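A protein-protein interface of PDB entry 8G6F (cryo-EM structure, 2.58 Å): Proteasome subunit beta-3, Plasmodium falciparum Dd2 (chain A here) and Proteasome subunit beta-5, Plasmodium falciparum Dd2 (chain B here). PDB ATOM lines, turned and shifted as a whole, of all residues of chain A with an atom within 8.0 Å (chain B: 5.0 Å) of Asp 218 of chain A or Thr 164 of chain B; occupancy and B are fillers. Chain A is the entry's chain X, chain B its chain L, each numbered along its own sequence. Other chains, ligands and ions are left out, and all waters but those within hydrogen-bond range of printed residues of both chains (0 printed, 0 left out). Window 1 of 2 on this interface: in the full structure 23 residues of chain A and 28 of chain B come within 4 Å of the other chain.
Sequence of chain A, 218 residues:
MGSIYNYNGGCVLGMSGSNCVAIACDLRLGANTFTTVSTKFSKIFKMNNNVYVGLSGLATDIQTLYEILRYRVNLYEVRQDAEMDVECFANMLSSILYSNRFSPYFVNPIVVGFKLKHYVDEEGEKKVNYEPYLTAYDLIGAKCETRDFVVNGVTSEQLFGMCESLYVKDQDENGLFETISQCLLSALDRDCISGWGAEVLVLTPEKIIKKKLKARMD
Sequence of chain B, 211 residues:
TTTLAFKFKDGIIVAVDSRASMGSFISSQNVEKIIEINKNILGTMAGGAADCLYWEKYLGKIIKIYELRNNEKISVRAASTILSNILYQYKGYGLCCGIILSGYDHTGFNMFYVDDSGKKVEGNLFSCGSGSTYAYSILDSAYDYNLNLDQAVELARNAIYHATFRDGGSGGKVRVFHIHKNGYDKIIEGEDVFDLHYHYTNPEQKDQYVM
The guanidinium group of Arg 19 of chain B is in hydrogen-bond range of the backbone carbonyl oxygen of Gly 168 of chain B, at 2.9 Å. The side-chain hydroxyl (OG1) of Thr 164 of chain B lies close to the backbone carbonyl oxygen (O) of Ile 160 of chain B. The backbone carbonyl oxygen of Gly 172 of chain B lies within hydrogen-bond range of the backbone NH of Val 193 of chain B. The guanidinium group (NE) of Arg 28 of chain A lies within hydrogen-bond range of the side-chain hydroxyl (OG1) of Thr 36 of chain A (3.1 Å). The backbone carbonyl oxygen (O) of Arg 216 of chain A lies within hydrogen-bond range of the backbone NH (N) of Trp 196 of chain A, 3.4 Å away. OG1 of Thr 2 of chain B lies within hydrogen-bond range of OG of Ser 170 of chain B (2.9 Å).
Asp 191 of chain A touches none of the printed residues of chain B. Gly 197 of chain A touches none of the printed residues of chain B. Of the printed residues of chain B, Met 217 of chain A touches Phe 165 (3.1 Å). Asp 218 of chain A touches just these residues of chain B: Arg 19 (2.9 Å), Thr 164 (2.9 Å), Asp 167 (3.1 Å), Ser 170 (2.9 Å), Gly 171 (3.8 Å), Gly 172 (3.6 Å) and Val 193 (3.3 Å). Ala 163 of chain B touches none of the printed residues of chain A. Thr 164 of chain B touches one residue of chain A. Of the printed residues of chain A, Asp 167 of chain B touches Phe 34 and Asp 218. Printed residues of chain A within 4 Å of Ser 170 of chain B: Asp 218 (2.9 Å). The nearest residue of chain B that does not touch Asp 218 of chain A is Gly 168 of chain B (4.2 Å). The nearest residue of chain A that does not touch Thr 164 of chain B is Met 217 of chain A (4.2 Å). The nearest printed residue of chain B that does not touch Thr 36 of chain A is Phe 165 of chain B (4.3 Å).
SG of Cys 192 of chain A sits close to O of Gly 168 of chain B (3.6 Å). The guanidinium group of Arg 166 of chain B sits at hydrogen-bond distance from the backbone carbonyl oxygen of Thr 36 of chain A, 2.7 Å away. O of Ser 170 of chain B sits close to OXT of Asp 218 of chain A (2.9 Å). The backbone carbonyl oxygen (O) of Phe 34 of chain A lies within hydrogen-bond range of the backbone NH (N) of Gly 168 of chain B, 3.0 Å away. NH2 of Arg 19 of chain B is in salt-bridge range of OD1 of Asp 218 of chain A. OXT of Asp 218 of chain A sits close to O of Asp 167 of chain B (3.1 Å). The chain-end carboxylate (OXT) of Asp 218 of chain A lies close to the backbone carbonyl oxygen (O) of Thr 164 of chain B. The indole nitrogen of Trp 196 of chain A is in hydrogen-bond range of the backbone carbonyl oxygen of Phe 165 of chain B. The guanidinium group (NH2) of Arg 216 of chain A is in hydrogen-bond range of the backbone carbonyl oxygen (O) of Gly 172 of chain B (3.5 Å).
Among the printed residues, pairs that only touch across the chains: Phe 34 of chain A with Arg 166 of chain B (3.6 Å), Phe 34 of chain A with Asp 167 of chain B (3.6 Å), Trp 196 of chain A with Gly 168 of chain B (3.7 Å), Arg 216 of chain A with Gln 29 of chain B (3.9 Å), Arg 216 of chain A with Val 193 of chain B (3.8 Å), Met 217 of chain A with Phe 165 of chain B (3.1 Å), Asp 218 of chain A with Gly 171 of chain B (3.8 Å), Asp 218 of chain A with Gly 172 of chain B (3.6 Å) and Asp 218 of chain A with Val 193 of chain B (3.3 Å).
Among the printed residues, 18 pairs touch across the chains.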
ATOM      1  N   ARG A  28      -3.833   3.466 -10.934  1.00  0.00           N
ATOM      2  CA  ARG A  28      -3.206   2.297 -11.530  1.00  0.00           C
ATOM      3  C   ARG A  28      -3.976   1.022 -11.205  1.00  0.00           C
ATOM      4  O   ARG A  28      -4.610   0.901 -10.154  1.00  0.00           O
ATOM      5  CB  ARG A  28      -1.770   2.162 -11.031  1.00  0.00           C
ATOM      6  CG  ARG A  28      -0.942   1.126 -11.759  1.00  0.00           C
ATOM      7  CD  ARG A  28      -0.282   0.153 -10.799  1.00  0.00           C
ATOM      8  NE  ARG A  28       0.931  -0.425 -11.362  1.00  0.00           N
ATOM      9  CZ  ARG A  28       1.540  -1.504 -10.890  1.00  0.00           C
ATOM     10  NH1 ARG A  28       1.067  -2.165  -9.847  1.00  0.00           N
ATOM     11  NH2 ARG A  28       2.653  -1.928 -11.474  1.00  0.00           N
ATOM     12  N   PHE A  34       4.025  -5.814 -10.406  1.00  0.00           N
ATOM     13  CA  PHE A  34       4.899  -4.943 -11.177  1.00  0.00           C
ATOM     14  C   PHE A  34       4.446  -4.697 -12.605  1.00  0.00           C
ATOM     15  O   PHE A  34       5.101  -3.920 -13.304  1.00  0.00           O
ATOM     16  CB  PHE A  34       6.328  -5.510 -11.195  1.00  0.00           C
ATOM     17  CG  PHE A  34       7.166  -5.094 -10.016  1.00  0.00           C
ATOM     18  CD1 PHE A  34       7.140  -3.794  -9.541  1.00  0.00           C
ATOM     19  CD2 PHE A  34       7.980  -6.009  -9.382  1.00  0.00           C
ATOM     20  CE1 PHE A  34       7.905  -3.420  -8.461  1.00  0.00           C
ATOM     21  CE2 PHE A  34       8.748  -5.636  -8.299  1.00  0.00           C
ATOM     22  CZ  PHE A  34       8.710  -4.340  -7.840  1.00  0.00           C
ATOM     23  N   THR A  36       1.705  -3.068 -15.080  1.00  0.00           N
ATOM     24  CA  THR A  36       0.603  -2.123 -15.153  1.00  0.00           C
ATOM     25  C   THR A  36      -0.274  -2.493 -16.337  1.00  0.00           C
ATOM     26  O   THR A  36       0.189  -2.494 -17.480  1.00  0.00           O
ATOM     27  CB  THR A  36       1.126  -0.697 -15.288  1.00  0.00           C
ATOM     28  OG1 THR A  36       2.044  -0.431 -14.224  1.00  0.00           O
ATOM     29  CG2 THR A  36      -0.010   0.304 -15.228  1.00  0.00           C
ATOM     30  N   LEU A 188       3.208   9.047  -3.764  1.00  0.00           N
ATOM     31  CA  LEU A 188       3.217   8.128  -4.894  1.00  0.00           C
ATOM     32  C   LEU A 188       4.578   8.073  -5.565  1.00  0.00           C
ATOM     33  O   LEU A 188       4.959   7.028  -6.102  1.00  0.00           O
ATOM     34  CB  LEU A 188       2.161   8.539  -5.917  1.00  0.00           C
ATOM     35  CG  LEU A 188       0.703   8.264  -5.568  1.00  0.00           C
ATOM     36  CD1 LEU A 188      -0.200   8.782  -6.673  1.00  0.00           C
ATOM     37  CD2 LEU A 188       0.473   6.791  -5.325  1.00  0.00           C
ATOM     38  N   ASP A 189       5.324   9.176  -5.550  1.00  0.00           N
ATOM     39  CA  ASP A 189       6.618   9.187  -6.217  1.00  0.00           C
ATOM     40  C   ASP A 189       7.597   8.200  -5.599  1.00  0.00           C
ATOM     41  O   ASP A 189       8.615   7.886  -6.223  1.00  0.00           O
ATOM     42  CB  ASP A 189       7.206  10.594  -6.182  1.00  0.00           C
ATOM     43  CG  ASP A 189       6.528  11.531  -7.157  1.00  0.00           C
ATOM     44  OD1 ASP A 189       5.519  11.128  -7.768  1.00  0.00           O
ATOM     45  OD2 ASP A 189       7.006  12.674  -7.315  1.00  0.00           O
ATOM     46  N   ASP A 191       6.634   5.053  -4.411  1.00  0.00           N
ATOM     47  CA  ASP A 191       6.048   3.719  -4.445  1.00  0.00           C
ATOM     48  C   ASP A 191       6.200   3.131  -5.837  1.00  0.00           C
ATOM     49  O   ASP A 191       5.869   3.784  -6.831  1.00  0.00           O
ATOM     50  CB  ASP A 191       4.570   3.756  -4.056  1.00  0.00           C
ATOM     51  CG  ASP A 191       4.130   2.511  -3.306  1.00  0.00           C
ATOM     52  OD1 ASP A 191       4.965   1.891  -2.613  1.00  0.00           O
ATOM     53  OD2 ASP A 191       2.947   2.139  -3.420  1.00  0.00           O
ATOM     54  N   CYS A 192       6.698   1.897  -5.907  1.00  0.00           N
ATOM     55  CA  CYS A 192       6.849   1.235  -7.197  1.00  0.00           C
ATOM     56  C   CYS A 192       5.502   0.809  -7.763  1.00  0.00           C
ATOM     57  O   CYS A 192       5.280   0.886  -8.976  1.00  0.00           O
ATOM     58  CB  CYS A 192       7.766   0.020  -7.058  1.00  0.00           C
ATOM     59  SG  CYS A 192       9.530   0.384  -7.074  1.00  0.00           S
ATOM     60  N   ILE A 193       4.591   0.367  -6.905  1.00  0.00           N
ATOM     61  CA  ILE A 193       3.378  -0.312  -7.330  1.00  0.00           C
ATOM     62  C   ILE A 193       2.150   0.590  -7.213  1.00  0.00           C
ATOM     63  O   ILE A 193       1.025   0.106  -7.261  1.00  0.00           O
ATOM     64  CB  ILE A 193       3.185  -1.619  -6.546  1.00  0.00           C
ATOM     65  CG1 ILE A 193       2.892  -1.322  -5.076  1.00  0.00           C
ATOM     66  CG2 ILE A 193       4.425  -2.470  -6.658  1.00  0.00           C
ATOM     67  CD1 ILE A 193       2.805  -2.545  -4.218  1.00  0.00           C
ATOM     68  N   SER A 194       2.345   1.895  -7.061  1.00  0.00           N
ATOM     69  CA  SER A 194       1.247   2.846  -7.019  1.00  0.00           C
ATOM     70  C   SER A 194       1.583   4.049  -7.884  1.00  0.00           C
ATOM     71  O   SER A 194       2.750   4.418  -8.033  1.00  0.00           O
ATOM     72  CB  SER A 194       0.950   3.304  -5.589  1.00  0.00           C
ATOM     73  OG  SER A 194       0.227   2.322  -4.874  1.00  0.00           O
ATOM     74  N   GLY A 195       0.548   4.657  -8.456  1.00  0.00           N
ATOM     75  CA  GLY A 195       0.730   5.848  -9.259  1.00  0.00           C
ATOM     76  C   GLY A 195       0.029   5.789 -10.597  1.00  0.00           C
ATOM     77  O   GLY A 195      -1.140   5.411 -10.676  1.00  0.00           O
ATOM     78  N   TRP A 196       0.740   6.164 -11.658  1.00  0.00           N
ATOM     79  CA  TRP A 196       0.188   6.173 -13.011  1.00  0.00           C
ATOM     80  C   TRP A 196      -1.092   7.002 -13.074  1.00  0.00           C
ATOM     81  O   TRP A 196      -2.090   6.606 -13.678  1.00  0.00           O
ATOM     82  CB  TRP A 196      -0.063   4.753 -13.507  1.00  0.00           C
ATOM     83  CG  TRP A 196       1.170   4.040 -13.952  1.00  0.00           C
ATOM     84  CD1 TRP A 196       1.680   4.000 -15.210  1.00  0.00           C
ATOM     85  CD2 TRP A 196       2.044   3.254 -13.137  1.00  0.00           C
ATOM     86  NE1 TRP A 196       2.818   3.239 -15.234  1.00  0.00           N
ATOM     87  CE2 TRP A 196       3.065   2.772 -13.971  1.00  0.00           C
ATOM     88  CE3 TRP A 196       2.063   2.914 -11.784  1.00  0.00           C
ATOM     89  CZ2 TRP A 196       4.091   1.965 -13.498  1.00  0.00           C
ATOM     90  CZ3 TRP A 196       3.079   2.120 -11.317  1.00  0.00           C
ATOM     91  CH2 TRP A 196       4.079   1.651 -12.169  1.00  0.00           C
ATOM     92  N   GLY A 197      -1.063   8.161 -12.445  1.00  0.00           N
ATOM     93  CA  GLY A 197      -2.195   9.059 -12.455  1.00  0.00           C
ATOM     94  C   GLY A 197      -2.853   9.149 -11.092  1.00  0.00           C
ATOM     95  O   GLY A 197      -2.902   8.180 -10.325  1.00  0.00           O
ATOM     96  N   ALA A 215       0.622  13.523 -13.317  1.00  0.00           N
ATOM     97  CA  ALA A 215       1.460  12.741 -12.421  1.00  0.00           C
ATOM     98  C   ALA A 215       2.505  11.973 -13.221  1.00  0.00           C
ATOM     99  O   ALA A 215       2.524  11.994 -14.451  1.00  0.00           O
ATOM    100  CB  ALA A 215       0.606  11.782 -11.588  1.00  0.00           C
ATOM    101  N   ARG A 216       3.393  11.300 -12.496  1.00  0.00           N
ATOM    102  CA  ARG A 216       4.373  10.424 -13.115  1.00  0.00           C
ATOM    103  C   ARG A 216       3.714   9.131 -13.573  1.00  0.00           C
ATOM    104  O   ARG A 216       2.774   8.633 -12.950  1.00  0.00           O
ATOM    105  CB  ARG A 216       5.503  10.106 -12.142  1.00  0.00           C
ATOM    106  CG  ARG A 216       6.288  11.311 -11.689  1.00  0.00           C
ATOM    107  CD  ARG A 216       7.484  10.894 -10.856  1.00  0.00           C
ATOM    108  NE  ARG A 216       8.516  10.262 -11.667  1.00  0.00           N
ATOM    109  CZ  ARG A 216       9.351  10.916 -12.461  1.00  0.00           C
ATOM    110  NH1 ARG A 216       9.318  12.234 -12.565  1.00  0.00           N
ATOM    111  NH2 ARG A 216      10.241  10.230 -13.170  1.00  0.00           N
ATOM    112  N   MET A 217       4.224   8.583 -14.670  1.00  0.00           N
ATOM    113  CA  MET A 217       3.695   7.362 -15.256  1.00  0.00           C
ATOM    114  C   MET A 217       4.802   6.340 -15.447  1.00  0.00           C
ATOM    115  O   MET A 217       4.866   5.653 -16.469  1.00  0.00           O
ATOM    116  CB  MET A 217       2.998   7.653 -16.583  1.00  0.00           C
ATOM    117  CG  MET A 217       2.055   8.846 -16.556  1.00  0.00           C
ATOM    118  SD  MET A 217       0.458   8.510 -15.798  1.00  0.00           S
ATOM    119  CE  MET A 217      -0.214   7.288 -16.910  1.00  0.00           C
ATOM    120  N   ASP A 218       5.690   6.218 -14.468  1.00  0.00           N
ATOM    121  CA  ASP A 218       6.789   5.265 -14.552  1.00  0.00           C
ATOM    122  C   ASP A 218       6.691   4.220 -13.445  1.00  0.00           C
ATOM    123  O   ASP A 218       6.040   4.440 -12.424  1.00  0.00           O
ATOM    124  CB  ASP A 218       8.138   5.986 -14.478  1.00  0.00           C
ATOM    125  CG  ASP A 218       8.192   7.016 -13.372  1.00  0.00           C
ATOM    126  OD1 ASP A 218       7.382   6.923 -12.430  1.00  0.00           O
ATOM    127  OD2 ASP A 218       9.049   7.918 -13.440  1.00  0.00           O
ATOM    128  OXT ASP A 218       7.258   3.132 -13.552  1.00  0.00           O
ATOM    129  N   THR B   2      15.750  -1.293 -16.404  1.00  0.00           N
ATOM    130  CA  THR B   2      15.827  -1.566 -17.829  1.00  0.00           C
ATOM    131  C   THR B   2      17.182  -1.093 -18.316  1.00  0.00           C
ATOM    132  O   THR B   2      17.505   0.095 -18.206  1.00  0.00           O
ATOM    133  CB  THR B   2      14.708  -0.874 -18.605  1.00  0.00           C
ATOM    134  OG1 THR B   2      13.494  -0.929 -17.850  1.00  0.00           O
ATOM    135  CG2 THR B   2      14.502  -1.559 -19.942  1.00  0.00           C
ATOM    136  N   ASP B  17      17.736   2.942 -17.387  1.00  0.00           N
ATOM    137  CA  ASP B  17      16.941   3.762 -16.484  1.00  0.00           C
ATOM    138  C   ASP B  17      17.750   4.067 -15.218  1.00  0.00           C
ATOM    139  O   ASP B  17      18.890   3.629 -15.062  1.00  0.00           O
ATOM    140  CB  ASP B  17      15.621   3.070 -16.150  1.00  0.00           C
ATOM    141  CG  ASP B  17      15.766   2.031 -15.060  1.00  0.00           C
ATOM    142  OD1 ASP B  17      16.611   1.128 -15.202  1.00  0.00           O
ATOM    143  OD2 ASP B  17      15.030   2.109 -14.059  1.00  0.00           O
ATOM    144  N   ARG B  19      16.303   3.936 -11.777  1.00  0.00           N
ATOM    145  CA  ARG B  19      15.528   3.643 -10.577  1.00  0.00           C
ATOM    146  C   ARG B  19      16.131   2.488  -9.786  1.00  0.00           C
ATOM    147  O   ARG B  19      16.531   1.470 -10.352  1.00  0.00           O
ATOM    148  CB  ARG B  19      14.076   3.314 -10.922  1.00  0.00           C
ATOM    149  CG  ARG B  19      13.234   2.938  -9.713  1.00  0.00           C
ATOM    150  CD  ARG B  19      11.770   2.790 -10.057  1.00  0.00           C
ATOM    151  NE  ARG B  19      11.154   4.064 -10.394  1.00  0.00           N
ATOM    152  CZ  ARG B  19       9.867   4.226 -10.660  1.00  0.00           C
ATOM    153  NH1 ARG B  19       9.025   3.210 -10.639  1.00  0.00           N
ATOM    154  NH2 ARG B  19       9.415   5.441 -10.950  1.00  0.00           N
ATOM    155  N   GLN B  29      15.990   7.364  -7.415  1.00  0.00           N
ATOM    156  CA  GLN B  29      15.617   7.560  -8.808  1.00  0.00           C
ATOM    157  C   GLN B  29      16.779   8.082  -9.640  1.00  0.00           C
ATOM    158  O   GLN B  29      16.576   8.445 -10.803  1.00  0.00           O
ATOM    159  CB  GLN B  29      14.437   8.530  -8.919  1.00  0.00           C
ATOM    160  CG  GLN B  29      13.122   7.997  -8.381  1.00  0.00           C
ATOM    161  CD  GLN B  29      12.175   7.553  -9.475  1.00  0.00           C
ATOM    162  OE1 GLN B  29      12.469   6.629 -10.224  1.00  0.00           O
ATOM    163  NE2 GLN B  29      11.032   8.216  -9.573  1.00  0.00           N
ATOM    164  N   ILE B 160      13.478   2.526 -23.637  1.00  0.00           N
ATOM    165  CA  ILE B 160      13.566   2.727 -22.194  1.00  0.00           C
ATOM    166  C   ILE B 160      12.281   3.350 -21.667  1.00  0.00           C
ATOM    167  O   ILE B 160      11.789   2.976 -20.596  1.00  0.00           O
ATOM    168  CB  ILE B 160      14.797   3.580 -21.836  1.00  0.00           C
ATOM    169  CG1 ILE B 160      16.092   2.813 -22.119  1.00  0.00           C
ATOM    170  CG2 ILE B 160      14.742   4.001 -20.378  1.00  0.00           C
ATOM    171  CD1 ILE B 160      16.299   1.581 -21.262  1.00  0.00           C
ATOM    172  N   TYR B 161      11.718   4.313 -22.398  1.00  0.00           N
ATOM    173  CA  TYR B 161      10.492   4.951 -21.938  1.00  0.00           C
ATOM    174  C   TYR B 161       9.362   3.940 -21.812  1.00  0.00           C
ATOM    175  O   TYR B 161       8.625   3.936 -20.821  1.00  0.00           O
ATOM    176  CB  TYR B 161      10.082   6.072 -22.886  1.00  0.00           C
ATOM    177  CG  TYR B 161       8.593   6.316 -22.866  1.00  0.00           C
ATOM    178  CD1 TYR B 161       7.976   6.850 -21.747  1.00  0.00           C
ATOM    179  CD2 TYR B 161       7.804   5.994 -23.953  1.00  0.00           C
ATOM    180  CE1 TYR B 161       6.622   7.062 -21.715  1.00  0.00           C
ATOM    181  CE2 TYR B 161       6.446   6.206 -23.930  1.00  0.00           C
ATOM    182  CZ  TYR B 161       5.861   6.740 -22.809  1.00  0.00           C
ATOM    183  OH  TYR B 161       4.507   6.953 -22.784  1.00  0.00           O
ATOM    184  N   HIS B 162       9.195   3.084 -22.818  1.00  0.00           N
ATOM    185  CA  HIS B 162       8.105   2.115 -22.769  1.00  0.00           C
ATOM    186  C   HIS B 162       8.326   1.094 -21.663  1.00  0.00           C
ATOM    187  O   HIS B 162       7.372   0.680 -20.988  1.00  0.00           O
ATOM    188  CB  HIS B 162       7.953   1.433 -24.125  1.00  0.00           C
ATOM    189  CG  HIS B 162       7.183   2.251 -25.111  1.00  0.00           C
ATOM    190  ND1 HIS B 162       5.828   2.468 -24.999  1.00  0.00           N
ATOM    191  CD2 HIS B 162       7.582   2.934 -26.207  1.00  0.00           C
ATOM    192  CE1 HIS B 162       5.424   3.236 -25.992  1.00  0.00           C
ATOM    193  NE2 HIS B 162       6.470   3.534 -26.739  1.00  0.00           N
ATOM    194  N   ALA B 163       9.577   0.680 -21.454  1.00  0.00           N
ATOM    195  CA  ALA B 163       9.860  -0.227 -20.351  1.00  0.00           C
ATOM    196  C   ALA B 163       9.496   0.407 -19.014  1.00  0.00           C
ATOM    197  O   ALA B 163       8.878  -0.241 -18.164  1.00  0.00           O
ATOM    198  CB  ALA B 163      11.329  -0.636 -20.374  1.00  0.00           C
ATOM    199  N   THR B 164       9.858   1.675 -18.812  1.00  0.00           N
ATOM    200  CA  THR B 164       9.501   2.352 -17.568  1.00  0.00           C
ATOM    201  C   THR B 164       7.992   2.490 -17.430  1.00  0.00           C
ATOM    202  O   THR B 164       7.446   2.358 -16.330  1.00  0.00           O
ATOM    203  CB  THR B 164      10.158   3.730 -17.489  1.00  0.00           C
ATOM    204  OG1 THR B 164       9.725   4.535 -18.589  1.00  0.00           O
ATOM    205  CG2 THR B 164      11.666   3.613 -17.504  1.00  0.00           C
ATOM    206  N   PHE B 165       7.302   2.772 -18.534  1.00  0.00           N
ATOM    207  CA  PHE B 165       5.858   2.955 -18.479  1.00  0.00           C
ATOM    208  C   PHE B 165       5.147   1.673 -18.071  1.00  0.00           C
ATOM    209  O   PHE B 165       4.198   1.711 -17.281  1.00  0.00           O
ATOM    210  CB  PHE B 165       5.344   3.441 -19.830  1.00  0.00           C
ATOM    211  CG  PHE B 165       3.885   3.784 -19.833  1.00  0.00           C
ATOM    212  CD1 PHE B 165       3.393   4.785 -19.018  1.00  0.00           C
ATOM    213  CD2 PHE B 165       3.004   3.106 -20.653  1.00  0.00           C
ATOM    214  CE1 PHE B 165       2.056   5.098 -19.019  1.00  0.00           C
ATOM    215  CE2 PHE B 165       1.667   3.420 -20.656  1.00  0.00           C
ATOM    216  CZ  PHE B 165       1.193   4.417 -19.837  1.00  0.00           C
ATOM    217  N   ARG B 166       5.579   0.531 -18.597  1.00  0.00           N
ATOM    218  CA  ARG B 166       4.878  -0.717 -18.318  1.00  0.00           C
ATOM    219  C   ARG B 166       5.369  -1.430 -17.066  1.00  0.00           C
ATOM    220  O   ARG B 166       4.618  -2.225 -16.493  1.00  0.00           O
ATOM    221  CB  ARG B 166       5.000  -1.671 -19.506  1.00  0.00           C
ATOM    222  CG  ARG B 166       3.951  -1.451 -20.570  1.00  0.00           C
ATOM    223  CD  ARG B 166       2.670  -2.187 -20.251  1.00  0.00           C
ATOM    224  NE  ARG B 166       1.630  -1.900 -21.230  1.00  0.00           N
ATOM    225  CZ  ARG B 166       0.383  -2.337 -21.152  1.00  0.00           C
ATOM    226  NH1 ARG B 166      -0.023  -3.095 -20.148  1.00  0.00           N
ATOM    227  NH2 ARG B 166      -0.480  -2.012 -22.109  1.00  0.00           N
ATOM    228  N   ASP B 167       6.595  -1.171 -16.624  1.00  0.00           N
ATOM    229  CA  ASP B 167       7.203  -1.890 -15.515  1.00  0.00           C
ATOM    230  C   ASP B 167       7.293  -0.983 -14.298  1.00  0.00           C
ATOM    231  O   ASP B 167       7.790   0.144 -14.394  1.00  0.00           O
ATOM    232  CB  ASP B 167       8.593  -2.395 -15.899  1.00  0.00           C
ATOM    233  CG  ASP B 167       9.307  -3.061 -14.752  1.00  0.00           C
ATOM    234  OD1 ASP B 167       8.628  -3.666 -13.901  1.00  0.00           O
ATOM    235  OD2 ASP B 167      10.549  -2.979 -14.699  1.00  0.00           O
ATOM    236  N   GLY B 168       6.820  -1.481 -13.155  1.00  0.00           N
ATOM    237  CA  GLY B 168       6.875  -0.709 -11.929  1.00  0.00           C
ATOM    238  C   GLY B 168       8.261  -0.592 -11.334  1.00  0.00           C
ATOM    239  O   GLY B 168       8.505   0.323 -10.544  1.00  0.00           O
ATOM    240  N   SER B 170      11.055   0.010 -13.035  1.00  0.00           N
ATOM    241  CA  SER B 170      11.884   0.891 -13.841  1.00  0.00           C
ATOM    242  C   SER B 170      11.281   2.286 -13.861  1.00  0.00           C
ATOM    243  O   SER B 170      10.060   2.452 -13.816  1.00  0.00           O
ATOM    244  CB  SER B 170      12.018   0.370 -15.272  1.00  0.00           C
ATOM    245  OG  SER B 170      12.059  -1.040 -15.302  1.00  0.00           O
ATOM    246  N   GLY B 171      12.145   3.289 -13.930  1.00  0.00           N
ATOM    247  CA  GLY B 171      11.682   4.661 -13.949  1.00  0.00           C
ATOM    248  C   GLY B 171      12.826   5.612 -13.679  1.00  0.00           C
ATOM    249  O   GLY B 171      13.994   5.244 -13.792  1.00  0.00           O
ATOM    250  N   GLY B 172      12.471   6.830 -13.324  1.00  0.00           N
ATOM    251  CA  GLY B 172      13.461   7.856 -12.999  1.00  0.00           C
ATOM    252  C   GLY B 172      13.917   8.614 -14.245  1.00  0.00           C
ATOM    253  O   GLY B 172      13.131   9.310 -14.868  1.00  0.00           O
ATOM    254  N   VAL B 193      11.705  10.696 -17.388  1.00  0.00           N
ATOM    255  CA  VAL B 193      10.674  10.071 -18.214  1.00  0.00           C
ATOM    256  C   VAL B 193       9.322  10.742 -18.049  1.00  0.00           C
ATOM    257  O   VAL B 193       8.392  10.449 -18.814  1.00  0.00           O
ATOM    258  CB  VAL B 193      10.567   8.565 -17.902  1.00  0.00           C
ATOM    259  CG1 VAL B 193      11.825   7.845 -18.351  1.00  0.00           C
ATOM    260  CG2 VAL B 193      10.318   8.326 -16.426  1.00  0.00           C
